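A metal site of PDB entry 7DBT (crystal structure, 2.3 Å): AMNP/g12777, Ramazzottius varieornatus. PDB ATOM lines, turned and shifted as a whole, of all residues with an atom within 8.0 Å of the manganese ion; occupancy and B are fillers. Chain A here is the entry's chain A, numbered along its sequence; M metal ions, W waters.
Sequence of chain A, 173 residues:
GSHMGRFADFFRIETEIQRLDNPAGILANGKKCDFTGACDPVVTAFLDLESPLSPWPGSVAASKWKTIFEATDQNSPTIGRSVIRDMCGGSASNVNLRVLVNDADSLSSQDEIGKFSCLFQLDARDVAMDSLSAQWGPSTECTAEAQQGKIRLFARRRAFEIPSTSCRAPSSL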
ATOM      1  N   CYS A  33       4.002   3.628  24.050  1.00  0.00           N
ATOM      2  CA  CYS A  33       3.209   2.650  23.313  1.00  0.00           C
ATOM      3  C   CYS A  33       4.089   1.575  22.701  1.00  0.00           C
ATOM      4  O   CYS A  33       3.901   0.374  22.940  1.00  0.00           O
ATOM      5  CB  CYS A  33       2.390   3.312  22.203  1.00  0.00           C
ATOM      6  SG  CYS A  33       1.097   4.438  22.666  1.00  0.00           S
ATOM      7  N   ASP A  34       5.037   2.000  21.868  1.00  0.00           N
ATOM      8  CA  ASP A  34       5.957   1.137  21.141  1.00  0.00           C
ATOM      9  C   ASP A  34       7.378   1.589  21.430  1.00  0.00           C
ATOM     10  O   ASP A  34       7.722   2.754  21.209  1.00  0.00           O
ATOM     11  CB  ASP A  34       5.673   1.186  19.629  1.00  0.00           C
ATOM     12  CG  ASP A  34       6.369   0.064  18.853  1.00  0.00           C
ATOM     13  OD1 ASP A  34       7.460  -0.383  19.256  1.00  0.00           O
ATOM     14  OD2 ASP A  34       5.793  -0.373  17.832  1.00  0.00           O
ATOM     15  N   PHE A  35       8.208   0.673  21.911  1.00  0.00           N
ATOM     16  CA  PHE A  35       9.550   1.093  22.259  1.00  0.00           C
ATOM     17  C   PHE A  35      10.480   1.234  21.044  1.00  0.00           C
ATOM     18  O   PHE A  35      11.510   1.900  21.152  1.00  0.00           O
ATOM     19  CB  PHE A  35      10.131   0.130  23.297  1.00  0.00           C
ATOM     20  CG  PHE A  35       9.524   0.295  24.667  1.00  0.00           C
ATOM     21  CD1 PHE A  35       9.750   1.445  25.405  1.00  0.00           C
ATOM     22  CD2 PHE A  35       8.697  -0.694  25.190  1.00  0.00           C
ATOM     23  CE1 PHE A  35       9.164   1.600  26.661  1.00  0.00           C
ATOM     24  CE2 PHE A  35       8.120  -0.536  26.450  1.00  0.00           C
ATOM     25  CZ  PHE A  35       8.352   0.606  27.179  1.00  0.00           C
ATOM     26  N   THR A  36      10.117   0.659  19.895  1.00  0.00           N
ATOM     27  CA  THR A  36      10.834   0.875  18.643  1.00  0.00           C
ATOM     28  C   THR A  36       9.990   1.570  17.572  1.00  0.00           C
ATOM     29  O   THR A  36      10.409   1.606  16.416  1.00  0.00           O
ATOM     30  CB  THR A  36      11.375  -0.449  18.077  1.00  0.00           C
ATOM     31  OG1 THR A  36      10.315  -1.167  17.431  1.00  0.00           O
ATOM     32  CG2 THR A  36      11.970  -1.309  19.181  1.00  0.00           C
ATOM     33  N   GLY A  37       8.817   2.072  17.923  1.00  0.00           N
ATOM     34  CA  GLY A  37       7.908   2.654  16.949  1.00  0.00           C
ATOM     35  C   GLY A  37       7.019   3.715  17.587  1.00  0.00           C
ATOM     36  O   GLY A  37       7.435   4.418  18.514  1.00  0.00           O
ATOM     37  N   ALA A  38       5.812   3.863  17.044  1.00  0.00           N
ATOM     38  CA  ALA A  38       4.811   4.812  17.540  1.00  0.00           C
ATOM     39  C   ALA A  38       3.563   4.074  18.030  1.00  0.00           C
ATOM     40  O   ALA A  38       3.401   2.859  17.860  1.00  0.00           O
ATOM     41  CB  ALA A  38       4.464   5.853  16.473  1.00  0.00           C
ATOM     42  N   CYS A  39       2.659   4.834  18.649  1.00  0.00           N
ATOM     43  CA  CYS A  39       1.367   4.276  19.027  1.00  0.00           C
ATOM     44  C   CYS A  39       0.610   3.774  17.796  1.00  0.00           C
ATOM     45  O   CYS A  39       0.828   4.244  16.676  1.00  0.00           O
ATOM     46  CB  CYS A  39       0.521   5.311  19.779  1.00  0.00           C
ATOM     47  SG  CYS A  39       1.271   5.948  21.346  1.00  0.00           S
ATOM     48  N   ASP A  40      -0.223   2.748  18.014  1.00  0.00           N
ATOM     49  CA  ASP A  40      -1.181   2.205  17.065  1.00  0.00           C
ATOM     50  C   ASP A  40      -2.577   2.511  17.576  1.00  0.00           C
ATOM     51  O   ASP A  40      -3.249   1.630  18.150  1.00  0.00           O
ATOM     52  CB  ASP A  40      -0.993   0.704  16.880  1.00  0.00           C
ATOM     53  CG  ASP A  40       0.359   0.347  16.342  1.00  0.00           C
ATOM     54  OD1 ASP A  40       1.093   1.266  15.932  1.00  0.00           O
ATOM     55  OD2 ASP A  40       0.683  -0.859  16.284  1.00  0.00           O
ATOM     56  N   PRO A  41      -3.049   3.745  17.409  1.00  0.00           N
ATOM     57  CA  PRO A  41      -4.277   4.165  18.110  1.00  0.00           C
ATOM     58  C   PRO A  41      -5.536   3.552  17.503  1.00  0.00           C
ATOM     59  O   PRO A  41      -5.716   3.539  16.279  1.00  0.00           O
ATOM     60  CB  PRO A  41      -4.249   5.693  17.962  1.00  0.00           C
ATOM     61  CG  PRO A  41      -3.436   5.932  16.711  1.00  0.00           C
ATOM     62  CD  PRO A  41      -2.418   4.842  16.652  1.00  0.00           C
ATOM     63  N   ALA A  71      -5.227   3.291  13.150  1.00  0.00           N
ATOM     64  CA  ALA A  71      -4.002   3.771  12.544  1.00  0.00           C
ATOM     65  C   ALA A  71      -2.830   2.975  13.103  1.00  0.00           C
ATOM     66  O   ALA A  71      -2.868   2.527  14.261  1.00  0.00           O
ATOM     67  CB  ALA A  71      -3.776   5.265  12.807  1.00  0.00           C
ATOM     68  N   THR A  72      -1.799   2.833  12.284  1.00  0.00           N
ATOM     69  CA  THR A  72      -0.590   2.127  12.675  1.00  0.00           C
ATOM     70  C   THR A  72       0.577   3.100  12.659  1.00  0.00           C
ATOM     71  O   THR A  72       0.801   3.791  11.664  1.00  0.00           O
ATOM     72  CB  THR A  72      -0.330   0.951  11.725  1.00  0.00           C
ATOM     73  OG1 THR A  72      -1.435   0.052  11.790  1.00  0.00           O
ATOM     74  CG2 THR A  72       0.938   0.215  12.148  1.00  0.00           C
ATOM     75  N   ASP A  73       1.328   3.133  13.759  1.00  0.00           N
ATOM     76  CA  ASP A  73       2.545   3.936  13.860  1.00  0.00           C
ATOM     77  C   ASP A  73       2.312   5.412  13.504  1.00  0.00           C
ATOM     78  O   ASP A  73       3.111   6.032  12.801  1.00  0.00           O
ATOM     79  CB  ASP A  73       3.667   3.344  13.010  1.00  0.00           C
ATOM     80  CG  ASP A  73       4.149   1.991  13.548  1.00  0.00           C
ATOM     81  OD1 ASP A  73       4.161   1.807  14.790  1.00  0.00           O
ATOM     82  OD2 ASP A  73       4.489   1.116  12.723  1.00  0.00           O
ATOM     83  N   GLN A  74       1.209   5.966  13.993  1.00  0.00           N
ATOM     84  CA  GLN A  74       0.983   7.417  13.945  1.00  0.00           C
ATOM     85  C   GLN A  74       0.589   7.901  15.335  1.00  0.00           C
ATOM     86  O   GLN A  74      -0.576   7.754  15.732  1.00  0.00           O
ATOM     87  CB  GLN A  74      -0.088   7.787  12.933  1.00  0.00           C
ATOM     88  CG  GLN A  74      -0.038   6.976  11.685  1.00  0.00           C
ATOM     89  CD  GLN A  74      -1.053   7.441  10.679  1.00  0.00           C
ATOM     90  OE1 GLN A  74      -1.569   8.549  10.760  1.00  0.00           O
ATOM     91  NE2 GLN A  74      -1.345   6.585   9.727  1.00  0.00           N
ATOM     92  N   ASN A  75       1.525   8.502  16.064  1.00  0.00           N
ATOM     93  CA  ASN A  75       1.210   9.028  17.385  1.00  0.00           C
ATOM     94  C   ASN A  75       0.111  10.074  17.325  1.00  0.00           C
ATOM     95  O   ASN A  75      -0.732  10.133  18.235  1.00  0.00           O
ATOM     96  CB  ASN A  75       2.455   9.614  18.058  1.00  0.00           C
ATOM     97  CG  ASN A  75       3.484   8.579  18.387  1.00  0.00           C
ATOM     98  OD1 ASN A  75       3.153   7.523  18.938  1.00  0.00           O
ATOM     99  ND2 ASN A  75       4.737   8.848  18.035  1.00  0.00           N
ATOM    100  N   ASP A 103      -4.004   1.548  22.268  1.00  0.00           N
ATOM    101  CA  ASP A 103      -2.881   1.162  21.417  1.00  0.00           C
ATOM    102  C   ASP A 103      -3.055  -0.277  20.942  1.00  0.00           C
ATOM    103  O   ASP A 103      -3.001  -1.211  21.745  1.00  0.00           O
ATOM    104  CB  ASP A 103      -1.577   1.346  22.175  1.00  0.00           C
ATOM    105  CG  ASP A 103      -0.378   0.829  21.413  1.00  0.00           C
ATOM    106  OD1 ASP A 103      -0.273   1.163  20.212  1.00  0.00           O
ATOM    107  OD2 ASP A 103       0.477   0.150  22.019  1.00  0.00           O
ATOM    108  N   ALA A 104      -3.197  -0.461  19.620  1.00  0.00           N
ATOM    109  CA  ALA A 104      -3.325  -1.789  18.995  1.00  0.00           C
ATOM    110  C   ALA A 104      -2.046  -2.607  19.070  1.00  0.00           C
ATOM    111  O   ALA A 104      -1.963  -3.592  19.811  1.00  0.00           O
ATOM    112  CB  ALA A 104      -3.761  -1.656  17.551  1.00  0.00           C
HETATM  113 MN    MN M   1       3.302   0.818  16.807  1.00  0.00          MN
HETATM  114  O   HOH W   1       2.282   0.448  19.456  1.00  0.00           O
HETATM  115  O   HOH W   2       3.171  -1.352  16.315  1.00  0.00           O
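The backbone carbonyl oxygen (O) of Asp 40 sits at hydrogen-bond distance from the backbone NH (N) of Ala 104 (2.6 Å). OD1 of Asp 34 is in hydrogen-bond range of N of Gly 37 (3.1 Å). N of Asp 40 lies within hydrogen-bond range of OD1 of Asp 103 (2.7 Å). The side-chain carboxylate (OD1) of Asp 34 lies within hydrogen-bond range of the backbone NH (N) of Thr 36. The side-chain sulfur (SG) of Cys 39 forms a disulfide with the side-chain sulfur (SG) of Cys 33 (2.0 Å). The backbone carbonyl oxygen of Cys 39 is in hydrogen-bond range of the backbone NH of Asp 73, 3.2 Å away.
The nearest printed residue that does not touch the manganese ion is Cys 39 (4.1 Å).
The manganese ion is bound by water W2 (2.2 Å), the backbone carbonyl oxygen (O) of Ala 38 (2.3 Å), the side-chain carboxylate (OD1) of Asp 73 (2.4 Å) and the side-chain carboxylate (OD1) of Asp 40 (2.4 Å). The manganese ion has four donor atoms within binding distance. Slightly farther from the manganese ion lies water W1 (2.9 Å). Slightly farther from the manganese ion lies OD2 of Asp 34 (2.9 Å).
Water W2 lies within hydrogen-bond range of the side-chain carboxylate of Asp 40 and the side-chain carboxylate of Asp 34.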
